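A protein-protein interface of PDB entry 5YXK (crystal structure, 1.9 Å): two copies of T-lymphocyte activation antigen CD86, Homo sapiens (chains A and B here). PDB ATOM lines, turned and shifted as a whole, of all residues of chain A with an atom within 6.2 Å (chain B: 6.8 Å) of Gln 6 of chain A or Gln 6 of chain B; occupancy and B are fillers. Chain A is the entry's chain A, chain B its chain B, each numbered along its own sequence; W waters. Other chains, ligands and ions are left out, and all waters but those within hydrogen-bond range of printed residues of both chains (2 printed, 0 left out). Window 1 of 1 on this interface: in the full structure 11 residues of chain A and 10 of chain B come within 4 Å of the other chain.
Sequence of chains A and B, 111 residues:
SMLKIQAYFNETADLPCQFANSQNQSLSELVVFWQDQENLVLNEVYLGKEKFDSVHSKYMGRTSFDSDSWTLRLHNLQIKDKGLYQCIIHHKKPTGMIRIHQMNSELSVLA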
ATOM      1  N   LYS A   4      14.651  22.357  18.912  1.00  0.00           N
ATOM      2  CA  LYS A   4      15.506  21.771  19.924  1.00  0.00           C
ATOM      3  C   LYS A   4      14.648  21.113  20.980  1.00  0.00           C
ATOM      4  O   LYS A   4      13.694  21.695  21.447  1.00  0.00           O
ATOM      5  CB  LYS A   4      16.415  22.826  20.540  1.00  0.00           C
ATOM      6  CG  LYS A   4      16.904  23.826  19.498  1.00  0.00           C
ATOM      7  CD  LYS A   4      18.400  24.013  19.593  1.00  0.00           C
ATOM      8  CE  LYS A   4      18.945  24.643  18.326  1.00  0.00           C
ATOM      9  NZ  LYS A   4      20.351  24.194  18.148  1.00  0.00           N
ATOM     10  N   ILE A   5      15.011  19.886  21.325  1.00  0.00           N
ATOM     11  CA  ILE A   5      14.292  19.068  22.266  1.00  0.00           C
ATOM     12  C   ILE A   5      15.262  18.643  23.337  1.00  0.00           C
ATOM     13  O   ILE A   5      16.364  18.157  23.027  1.00  0.00           O
ATOM     14  CB  ILE A   5      13.778  17.778  21.602  1.00  0.00           C
ATOM     15  CG1 ILE A   5      12.954  18.096  20.358  1.00  0.00           C
ATOM     16  CG2 ILE A   5      12.975  16.916  22.589  1.00  0.00           C
ATOM     17  CD1 ILE A   5      11.562  18.545  20.687  1.00  0.00           C
ATOM     18  N   GLN A   6      14.875  18.835  24.597  1.00  0.00           N
ATOM     19  CA  GLN A   6      15.683  18.367  25.698  1.00  0.00           C
ATOM     20  C   GLN A   6      14.912  17.240  26.384  1.00  0.00           C
ATOM     21  O   GLN A   6      13.752  17.412  26.816  1.00  0.00           O
ATOM     22  CB  GLN A   6      16.034  19.512  26.646  1.00  0.00           C
ATOM     23  CG  GLN A   6      16.719  19.109  27.934  1.00  0.00           C
ATOM     24  CD  GLN A   6      16.859  20.287  28.872  1.00  0.00           C
ATOM     25  OE1 GLN A   6      17.542  21.252  28.551  1.00  0.00           O
ATOM     26  NE2 GLN A   6      16.182  20.236  30.001  1.00  0.00           N
ATOM     27  N   ALA A   7      15.521  16.064  26.427  1.00  0.00           N
ATOM     28  CA  ALA A   7      14.882  14.911  27.026  1.00  0.00           C
ATOM     29  C   ALA A   7      15.818  14.228  28.020  1.00  0.00           C
ATOM     30  O   ALA A   7      16.908  14.693  28.230  1.00  0.00           O
ATOM     31  CB  ALA A   7      14.436  13.938  25.923  1.00  0.00           C
ATOM     32  N   TYR A   8      15.392  13.125  28.640  1.00  0.00           N
ATOM     33  CA  TYR A   8      16.175  12.527  29.723  1.00  0.00           C
ATOM     34  C   TYR A   8      16.549  11.063  29.557  1.00  0.00           C
ATOM     35  O   TYR A   8      15.784  10.268  29.068  1.00  0.00           O
ATOM     36  CB  TYR A   8      15.469  12.741  31.071  1.00  0.00           C
ATOM     37  CG  TYR A   8      15.466  14.196  31.459  1.00  0.00           C
ATOM     38  CD1 TYR A   8      14.492  15.075  30.951  1.00  0.00           C
ATOM     39  CD2 TYR A   8      16.466  14.713  32.261  1.00  0.00           C
ATOM     40  CE1 TYR A   8      14.512  16.422  31.273  1.00  0.00           C
ATOM     41  CE2 TYR A   8      16.489  16.050  32.595  1.00  0.00           C
ATOM     42  CZ  TYR A   8      15.512  16.893  32.104  1.00  0.00           C
ATOM     43  OH  TYR A   8      15.552  18.212  32.444  1.00  0.00           O
ATOM     44  N   GLU A  11      14.408   7.712  29.484  1.00  0.00           N
ATOM     45  CA  GLU A  11      13.046   8.124  29.281  1.00  0.00           C
ATOM     46  C   GLU A  11      12.848   8.223  27.790  1.00  0.00           C
ATOM     47  O   GLU A  11      13.483   7.477  27.046  1.00  0.00           O
ATOM     48  CB  GLU A  11      12.781   9.468  29.972  1.00  0.00           C
ATOM     49  CG  GLU A  11      13.138   9.476  31.449  1.00  0.00           C
ATOM     50  CD  GLU A  11      12.124   8.739  32.296  1.00  0.00           C
ATOM     51  OE1 GLU A  11      11.899   9.179  33.445  1.00  0.00           O
ATOM     52  OE2 GLU A  11      11.530   7.738  31.823  1.00  0.00           O
ATOM     53  N   THR A  12      12.014   9.162  27.343  1.00  0.00           N
ATOM     54  CA  THR A  12      11.573   9.165  25.945  1.00  0.00           C
ATOM     55  C   THR A  12      11.875  10.492  25.225  1.00  0.00           C
ATOM     56  O   THR A  12      12.017  11.543  25.858  1.00  0.00           O
ATOM     57  CB  THR A  12      10.053   8.887  25.845  1.00  0.00           C
ATOM     58  OG1 THR A  12       9.318   9.890  26.571  1.00  0.00           O
ATOM     59  CG2 THR A  12       9.690   7.506  26.424  1.00  0.00           C
ATOM     60  N   ALA A  13      11.985  10.432  23.898  1.00  0.00           N
ATOM     61  CA  ALA A  13      11.924  11.655  23.103  1.00  0.00           C
ATOM     62  C   ALA A  13      10.801  11.584  22.068  1.00  0.00           C
ATOM     63  O   ALA A  13      10.648  10.591  21.337  1.00  0.00           O
ATOM     64  CB  ALA A  13      13.264  11.926  22.438  1.00  0.00           C
ATOM     65  N   ASP A  14      10.023  12.655  21.990  1.00  0.00           N
ATOM     66  CA  ASP A  14       9.029  12.785  20.947  1.00  0.00           C
ATOM     67  C   ASP A  14       9.492  13.793  19.885  1.00  0.00           C
ATOM     68  O   ASP A  14       9.599  14.987  20.149  1.00  0.00           O
ATOM     69  CB  ASP A  14       7.678  13.166  21.569  1.00  0.00           C
ATOM     70  CG  ASP A  14       7.117  12.050  22.456  1.00  0.00           C
ATOM     71  OD1 ASP A  14       6.962  10.915  21.949  1.00  0.00           O
ATOM     72  OD2 ASP A  14       6.834  12.278  23.660  1.00  0.00           O
ATOM     73  N   LEU A  15       9.836  13.289  18.707  1.00  0.00           N
ATOM     74  CA  LEU A  15      10.288  14.139  17.595  1.00  0.00           C
ATOM     75  C   LEU A  15       9.146  14.338  16.570  1.00  0.00           C
ATOM     76  O   LEU A  15       8.535  13.383  16.135  1.00  0.00           O
ATOM     77  CB  LEU A  15      11.517  13.527  16.915  1.00  0.00           C
ATOM     78  CG  LEU A  15      12.665  12.945  17.742  1.00  0.00           C
ATOM     79  CD1 LEU A  15      13.673  12.215  16.857  1.00  0.00           C
ATOM     80  CD2 LEU A  15      13.395  14.033  18.506  1.00  0.00           C
ATOM     81  N   GLU A 106      17.001  18.799  16.961  1.00  0.00           N
ATOM     82  CA  GLU A 106      18.217  18.479  17.674  1.00  0.00           C
ATOM     83  C   GLU A 106      17.840  18.015  19.053  1.00  0.00           C
ATOM     84  O   GLU A 106      17.142  18.739  19.779  1.00  0.00           O
ATOM     85  CB  GLU A 106      19.139  19.678  17.805  1.00  0.00           C
ATOM     86  CG  GLU A 106      20.316  19.356  18.715  1.00  0.00           C
ATOM     87  CD  GLU A 106      21.479  20.262  18.490  1.00  0.00           C
ATOM     88  OE1 GLU A 106      21.245  21.489  18.420  1.00  0.00           O
ATOM     89  OE2 GLU A 106      22.611  19.746  18.386  1.00  0.00           O
ATOM     90  N   LEU A 107      18.327  16.829  19.427  1.00  0.00           N
ATOM     91  CA  LEU A 107      17.987  16.259  20.710  1.00  0.00           C
ATOM     92  C   LEU A 107      19.146  16.354  21.666  1.00  0.00           C
ATOM     93  O   LEU A 107      20.258  15.974  21.306  1.00  0.00           O
ATOM     94  CB  LEU A 107      17.583  14.802  20.536  1.00  0.00           C
ATOM     95  CG  LEU A 107      17.244  13.994  21.793  1.00  0.00           C
ATOM     96  CD1 LEU A 107      16.023  14.563  22.493  1.00  0.00           C
ATOM     97  CD2 LEU A 107      17.006  12.558  21.408  1.00  0.00           C
ATOM     98  N   SER A 108      18.885  16.890  22.865  1.00  0.00           N
ATOM     99  CA  SER A 108      19.765  16.678  24.043  1.00  0.00           C
ATOM    100  C   SER A 108      19.201  15.613  24.966  1.00  0.00           C
ATOM    101  O   SER A 108      17.994  15.536  25.204  1.00  0.00           O
ATOM    102  CB  SER A 108      19.905  17.942  24.876  1.00  0.00           C
ATOM    103  OG  SER A 108      20.055  19.053  24.056  1.00  0.00           O
ATOM    104  N   VAL A 109      20.093  14.775  25.498  1.00  0.00           N
ATOM    105  CA  VAL A 109      19.707  13.776  26.455  1.00  0.00           C
ATOM    106  C   VAL A 109      20.439  14.126  27.724  1.00  0.00           C
ATOM    107  O   VAL A 109      21.661  14.078  27.765  1.00  0.00           O
ATOM    108  CB  VAL A 109      20.096  12.356  26.005  1.00  0.00           C
ATOM    109  CG1 VAL A 109      19.554  11.341  26.992  1.00  0.00           C
ATOM    110  CG2 VAL A 109      19.580  12.065  24.584  1.00  0.00           C
ATOM    111  N   LEU A 110      19.711  14.527  28.753  1.00  0.00           N
ATOM    112  CA  LEU A 110      20.364  14.884  30.017  1.00  0.00           C
ATOM    113  C   LEU A 110      20.435  13.667  30.944  1.00  0.00           C
ATOM    114  O   LEU A 110      19.543  12.801  30.924  1.00  0.00           O
ATOM    115  CB  LEU A 110      19.610  16.025  30.716  1.00  0.00           C
ATOM    116  CG  LEU A 110      19.732  17.393  30.030  1.00  0.00           C
ATOM    117  CD1 LEU A 110      19.032  18.507  30.814  1.00  0.00           C
ATOM    118  CD2 LEU A 110      21.193  17.704  29.844  1.00  0.00           C
ATOM    119  N   LEU B   3      13.194  26.105  23.402  1.00  0.00           N
ATOM    120  CA  LEU B   3      13.577  24.753  23.775  1.00  0.00           C
ATOM    121  C   LEU B   3      12.366  23.967  24.258  1.00  0.00           C
ATOM    122  O   LEU B   3      11.585  24.482  25.067  1.00  0.00           O
ATOM    123  CB  LEU B   3      14.586  24.868  24.907  1.00  0.00           C
ATOM    124  CG  LEU B   3      15.164  23.586  25.462  1.00  0.00           C
ATOM    125  CD1 LEU B   3      15.931  22.882  24.360  1.00  0.00           C
ATOM    126  CD2 LEU B   3      16.048  23.961  26.639  1.00  0.00           C
ATOM    127  N   LYS B   4      12.195  22.739  23.754  1.00  0.00           N
ATOM    128  CA  LYS B   4      11.116  21.854  24.197  1.00  0.00           C
ATOM    129  C   LYS B   4      11.676  20.831  25.166  1.00  0.00           C
ATOM    130  O   LYS B   4      12.529  20.013  24.805  1.00  0.00           O
ATOM    131  CB  LYS B   4      10.490  21.133  23.014  1.00  0.00           C
ATOM    132  CG  LYS B   4       9.762  22.053  22.070  1.00  0.00           C
ATOM    133  CD  LYS B   4       9.117  21.293  20.919  1.00  0.00           C
ATOM    134  CE  LYS B   4       7.662  21.711  20.748  1.00  0.00           C
ATOM    135  NZ  LYS B   4       6.796  21.221  21.857  1.00  0.00           N
ATOM    136  N   ILE B   5      11.252  20.923  26.412  1.00  0.00           N
ATOM    137  CA  ILE B   5      11.782  20.058  27.470  1.00  0.00           C
ATOM    138  C   ILE B   5      10.737  18.989  27.742  1.00  0.00           C
ATOM    139  O   ILE B   5       9.542  19.297  27.969  1.00  0.00           O
ATOM    140  CB  ILE B   5      12.070  20.841  28.769  1.00  0.00           C
ATOM    141  CG1 ILE B   5      12.990  22.031  28.514  1.00  0.00           C
ATOM    142  CG2 ILE B   5      12.634  19.909  29.841  1.00  0.00           C
ATOM    143  CD1 ILE B   5      13.163  22.947  29.712  1.00  0.00           C
ATOM    144  N   GLN B   6      11.146  17.719  27.661  1.00  0.00           N
ATOM    145  CA  GLN B   6      10.220  16.637  27.884  1.00  0.00           C
ATOM    146  C   GLN B   6      10.668  15.852  29.098  1.00  0.00           C
ATOM    147  O   GLN B   6      11.635  15.098  29.040  1.00  0.00           O
ATOM    148  CB  GLN B   6      10.170  15.737  26.653  1.00  0.00           C
ATOM    149  CG  GLN B   6       9.663  16.459  25.426  1.00  0.00           C
ATOM    150  CD  GLN B   6       9.800  15.658  24.143  1.00  0.00           C
ATOM    151  OE1 GLN B   6      10.324  14.541  24.144  1.00  0.00           O
ATOM    152  NE2 GLN B   6       9.364  16.244  23.029  1.00  0.00           N
ATOM    153  N   ALA B   7       9.992  16.038  30.209  1.00  0.00           N
ATOM    154  CA  ALA B   7      10.439  15.379  31.429  1.00  0.00           C
ATOM    155  C   ALA B   7       9.244  14.721  32.090  1.00  0.00           C
ATOM    156  O   ALA B   7       8.112  14.925  31.674  1.00  0.00           O
ATOM    157  CB  ALA B   7      11.102  16.376  32.351  1.00  0.00           C
ATOM    158  N   TYR B   8       9.495  13.933  33.129  1.00  0.00           N
ATOM    159  CA  TYR B   8       8.458  13.049  33.657  1.00  0.00           C
ATOM    160  C   TYR B   8       7.968  13.423  35.061  1.00  0.00           C
ATOM    161  O   TYR B   8       8.713  13.960  35.862  1.00  0.00           O
ATOM    162  CB  TYR B   8       8.967  11.593  33.619  1.00  0.00           C
ATOM    163  CG  TYR B   8       8.740  10.955  32.273  1.00  0.00           C
ATOM    164  CD1 TYR B   8       9.469  11.354  31.141  1.00  0.00           C
ATOM    165  CD2 TYR B   8       7.777   9.969  32.115  1.00  0.00           C
ATOM    166  CE1 TYR B   8       9.230  10.780  29.907  1.00  0.00           C
ATOM    167  CE2 TYR B   8       7.535   9.391  30.887  1.00  0.00           C
ATOM    168  CZ  TYR B   8       8.253   9.792  29.787  1.00  0.00           C
ATOM    169  OH  TYR B   8       7.963   9.196  28.580  1.00  0.00           O
ATOM    170  N   ALA B  13      13.089  18.878  36.305  1.00  0.00           N
ATOM    171  CA  ALA B  13      13.313  19.508  34.980  1.00  0.00           C
ATOM    172  C   ALA B  13      14.472  20.454  35.150  1.00  0.00           C
ATOM    173  O   ALA B  13      14.614  21.078  36.222  1.00  0.00           O
ATOM    174  CB  ALA B  13      12.076  20.262  34.493  1.00  0.00           C
ATOM    175  N   ASP B  14      15.345  20.497  34.146  1.00  0.00           N
ATOM    176  CA  ASP B  14      16.456  21.444  34.112  1.00  0.00           C
ATOM    177  C   ASP B  14      16.038  22.580  33.212  1.00  0.00           C
ATOM    178  O   ASP B  14      15.841  22.369  32.009  1.00  0.00           O
ATOM    179  CB  ASP B  14      17.700  20.819  33.537  1.00  0.00           C
ATOM    180  CG  ASP B  14      18.195  19.692  34.355  1.00  0.00           C
ATOM    181  OD1 ASP B  14      17.608  18.597  34.249  1.00  0.00           O
ATOM    182  OD2 ASP B  14      19.181  19.899  35.073  1.00  0.00           O
ATOM    183  N   LEU B  15      15.883  23.764  33.791  1.00  0.00           N
ATOM    184  CA  LEU B  15      15.502  24.960  33.051  1.00  0.00           C
ATOM    185  C   LEU B  15      16.727  25.852  32.803  1.00  0.00           C
ATOM    186  O   LEU B  15      17.180  26.544  33.717  1.00  0.00           O
ATOM    187  CB  LEU B  15      14.447  25.736  33.836  1.00  0.00           C
ATOM    188  CG  LEU B  15      13.201  24.966  34.292  1.00  0.00           C
ATOM    189  CD1 LEU B  15      12.319  25.841  35.186  1.00  0.00           C
ATOM    190  CD2 LEU B  15      12.385  24.439  33.113  1.00  0.00           C
ATOM    191  N   PRO B  16      17.276  25.831  31.573  1.00  0.00           N
ATOM    192  CA  PRO B  16      18.614  26.391  31.356  1.00  0.00           C
ATOM    193  C   PRO B  16      18.562  27.846  30.945  1.00  0.00           C
ATOM    194  O   PRO B  16      17.545  28.308  30.435  1.00  0.00           O
ATOM    195  CB  PRO B  16      19.153  25.565  30.201  1.00  0.00           C
ATOM    196  CG  PRO B  16      17.942  25.187  29.429  1.00  0.00           C
ATOM    197  CD  PRO B  16      16.759  25.197  30.352  1.00  0.00           C
ATOM    198  N   GLN B  18      21.367  28.738  29.036  1.00  0.00           N
ATOM    199  CA  GLN B  18      22.201  28.681  27.819  1.00  0.00           C
ATOM    200  C   GLN B  18      22.844  30.044  27.485  1.00  0.00           C
ATOM    201  O   GLN B  18      22.559  30.667  26.440  1.00  0.00           O
ATOM    202  CB  GLN B  18      21.394  28.158  26.636  1.00  0.00           C
ATOM    203  CG  GLN B  18      21.642  26.687  26.381  1.00  0.00           C
ATOM    204  CD  GLN B  18      20.544  26.016  25.605  1.00  0.00           C
ATOM    205  OE1 GLN B  18      20.053  26.531  24.589  1.00  0.00           O
ATOM    206  NE2 GLN B  18      20.174  24.833  26.056  1.00  0.00           N
ATOM    207  N   SER B 105      11.840  28.356  27.477  1.00  0.00           N
ATOM    208  CA  SER B 105      11.743  26.911  27.434  1.00  0.00           C
ATOM    209  C   SER B 105      10.286  26.504  27.667  1.00  0.00           C
ATOM    210  O   SER B 105       9.557  27.122  28.467  1.00  0.00           O
ATOM    211  CB  SER B 105      12.633  26.303  28.529  1.00  0.00           C
ATOM    212  OG  SER B 105      14.015  26.629  28.325  1.00  0.00           O
ATOM    213  N   GLU B 106       9.862  25.466  26.973  1.00  0.00           N
ATOM    214  CA  GLU B 106       8.519  24.912  27.205  1.00  0.00           C
ATOM    215  C   GLU B 106       8.685  23.573  27.896  1.00  0.00           C
ATOM    216  O   GLU B 106       9.413  22.695  27.418  1.00  0.00           O
ATOM    217  CB  GLU B 106       7.733  24.725  25.916  1.00  0.00           C
ATOM    218  CG  GLU B 106       6.442  23.941  26.154  1.00  0.00           C
ATOM    219  CD  GLU B 106       5.854  23.331  24.903  1.00  0.00           C
ATOM    220  OE1 GLU B 106       4.745  23.786  24.525  1.00  0.00           O
ATOM    221  OE2 GLU B 106       6.472  22.400  24.307  1.00  0.00           O
ATOM    222  N   LEU B 107       8.037  23.414  29.032  1.00  0.00           N
ATOM    223  CA  LEU B 107       8.146  22.183  29.732  1.00  0.00           C
ATOM    224  C   LEU B 107       6.900  21.375  29.492  1.00  0.00           C
ATOM    225  O   LEU B 107       5.802  21.894  29.692  1.00  0.00           O
ATOM    226  CB  LEU B 107       8.285  22.436  31.221  1.00  0.00           C
ATOM    227  CG  LEU B 107       8.378  21.197  32.095  1.00  0.00           C
ATOM    228  CD1 LEU B 107       9.566  20.340  31.683  1.00  0.00           C
ATOM    229  CD2 LEU B 107       8.499  21.629  33.541  1.00  0.00           C
ATOM    230  N   SER B 108       7.088  20.122  29.077  1.00  0.00           N
ATOM    231  CA  SER B 108       6.048  19.101  29.110  1.00  0.00           C
ATOM    232  C   SER B 108       6.352  18.109  30.216  1.00  0.00           C
ATOM    233  O   SER B 108       7.516  17.720  30.446  1.00  0.00           O
ATOM    234  CB  SER B 108       5.986  18.336  27.788  1.00  0.00           C
ATOM    235  OG  SER B 108       5.774  19.213  26.708  1.00  0.00           O
ATOM    236  N   VAL B 109       5.311  17.692  30.918  1.00  0.00           N
ATOM    237  CA  VAL B 109       5.484  16.670  31.929  1.00  0.00           C
ATOM    238  C   VAL B 109       4.720  15.404  31.576  1.00  0.00           C
ATOM    239  O   VAL B 109       3.511  15.413  31.592  1.00  0.00           O
ATOM    240  CB  VAL B 109       5.074  17.168  33.323  1.00  0.00           C
ATOM    241  CG1 VAL B 109       5.456  16.127  34.366  1.00  0.00           C
ATOM    242  CG2 VAL B 109       5.753  18.490  33.632  1.00  0.00           C
ATOM    243  N   LEU B 110       5.449  14.311  31.328  1.00  0.00           N
ATOM    244  CA  LEU B 110       4.861  13.044  30.866  1.00  0.00           C
ATOM    245  C   LEU B 110       4.904  11.925  31.935  1.00  0.00           C
ATOM    246  O   LEU B 110       5.479  12.097  33.007  1.00  0.00           O
ATOM    247  CB  LEU B 110       5.602  12.566  29.625  1.00  0.00           C
ATOM    248  CG  LEU B 110       5.795  13.620  28.535  1.00  0.00           C
ATOM    249  CD1 LEU B 110       6.711  13.047  27.471  1.00  0.00           C
ATOM    250  CD2 LEU B 110       4.446  14.072  27.964  1.00  0.00           C
HETATM  251  O   HOH W   1      12.597  12.676  28.459  1.00  0.00           O
HETATM  252  O   HOH W   2       9.096  12.197  25.314  1.00  0.00           O
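Ile 5 of chain A touches Lys 4 of chain B, but with the chains exchanged Lys 4 of chain A does not touch Ile 5 of chain B (5.6 Å). Gln 6 of chain A touches Asp 14 of chain B, and with the chains exchanged Asp 14 of chain A touches Gln 6 of chain B. Ala 7 of chain A touches Gln 6 of chain B, but with the chains exchanged Gln 6 of chain A does not touch Ala 7 of chain B (5.2 Å). Tyr 8 of chain A touches Asp 14 of chain B, but with the chains exchanged Asp 14 of chain A does not touch Tyr 8 of chain B (5.9 Å). Positions printed for both chains: 4, 5, 6, 7, 8, 13, 14, 15, 106, 107, 108, 109 and 110. Of the 21 pairs that touch across the chains among the printed residues, 8 have their exchanged pair printed and touching as well.
Printed residues of chain B that touch a printed residue of chain A: Leu 3, Lys 4, Ile 5, Gln 6, Ala 7, Tyr 8, Ala 13, Asp 14 and Leu 110. Hydrophobic or aromatic side chains of chain A that line the printed part of chain B: Ile 5, Tyr 8 and Leu 110. Among the printed residues, no Asp or Glu carboxylate lies within 4 Å of a Lys or Arg side-chain nitrogen of the other chain.
Gln 6 of chain A touches just these residues of chain B: Leu 3, Lys 4, Ile 5, Gln 6 and Asp 14. Of the printed residues of chain B, Tyr 8 of chain A touches Gln 6, Ala 7, Ala 13 and Asp 14. Of the printed residues of chain B, Leu 110 of chain A touches Asp 14 (3.7 Å). Of chain A, only Ile 5, Gln 6, Ala 7, Tyr 8, Thr 12, Ala 13 and Asp 14 come within 4 Å of Gln 6 of chain B. The nearest residue of chain B that does not touch Gln 6 of chain A is Pro 16 of chain B (4.1 Å). The nearest printed residue of chain B that does not touch Thr 12 of chain A is Leu 110 of chain B (4.2 Å).
The backbone NH (N) of Ala 7 of chain B lies within hydrogen-bond range of the backbone carbonyl oxygen (O) of Ser 108 of chain B, 3.0 Å away. The side-chain amino group of Lys 4 of chain A is in salt-bridge range of the side-chain carboxylate of Glu 106 of chain A (2.9 Å). The side-chain amino group (NZ) of Lys 4 of chain B is in salt-bridge range of the side-chain carboxylate (OE2) of Glu 106 of chain B (2.7 Å). The backbone carbonyl oxygen (O) of Ile 5 of chain B lies within hydrogen-bond range of the backbone NH (N) of Ser 108 of chain B (2.8 Å). O of Leu 3 of chain B is in hydrogen-bond range of N of Glu 106 of chain B, at 2.8 Å. The backbone carbonyl oxygen (O) of Glu 106 of chain A lies within hydrogen-bond range of the backbone NH (N) of Ile 5 of chain A, 2.9 Å away.
Among the printed residues, pairs that only touch across the chains: Ile 5 of chain A with Lys 4 of chain B (3.2 Å), Gln 6 of chain A with Ile 5 of chain B (3.4 Å), Tyr 8 of chain A with Gln 6 of chain B (3.4 Å), Ala 13 of chain A with Gln 6 of chain B (3.5 Å), Tyr 8 of chain A with Ala 7 of chain B (3.6 Å), Tyr 8 of chain A with Ala 13 of chain B (3.6 Å), Gln 6 of chain A with Leu 3 of chain B (3.6 Å), Ile 5 of chain A with Gln 6 of chain B (3.7 Å), Leu 110 of chain A with Asp 14 of chain B (3.7 Å), Glu 11 of chain A with Tyr 8 of chain B (3.8 Å), Ala 7 of chain A with Gln 6 of chain B (3.8 Å), Lys 4 of chain A with Leu 3 of chain B (3.8 Å), Thr 12 of chain A with Gln 6 of chain B (3.8 Å) and Asp 14 of chain A with Leu 110 of chain B (3.9 Å).
The backbone carbonyl oxygen of Lys 4 of chain A lies within hydrogen-bond range of the backbone NH of Lys 4 of chain B (2.9 Å). OH of Tyr 8 of chain A lies within hydrogen-bond range of OD1 of Asp 14 of chain B (2.8 Å). N of Gln 6 of chain B lies within hydrogen-bond range of O of Gln 6 of chain A, 2.8 Å away. NE2 of Gln 6 of chain A is in hydrogen-bond range of O of Asp 14 of chain B (2.9 Å). N of Gln 6 of chain A sits at hydrogen-bond distance from O of Lys 4 of chain B (2.6 Å). OG1 of Thr 12 of chain A sits at hydrogen-bond distance from OH of Tyr 8 of chain B (2.5 Å). OE1 of Gln 6 of chain B is in hydrogen-bond range of N of Asp 14 of chain A (2.9 Å).
Water W2 lies within hydrogen-bond range of the side-chain hydroxyl (OG1) of Thr 12 of chain A (2.6 Å), the side-chain carboxylate (OD2) of Asp 14 of chain A (2.8 Å) and the side-chain amide oxygen (OE1) of Gln 6 of chain B (2.9 Å). Water W1 lies within hydrogen-bond range of the backbone carbonyl oxygen (O) of Gln 6 of chain B, the backbone NH (N) of Tyr 8 of chain A and the backbone carbonyl oxygen (O) of Thr 12 of chain A.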
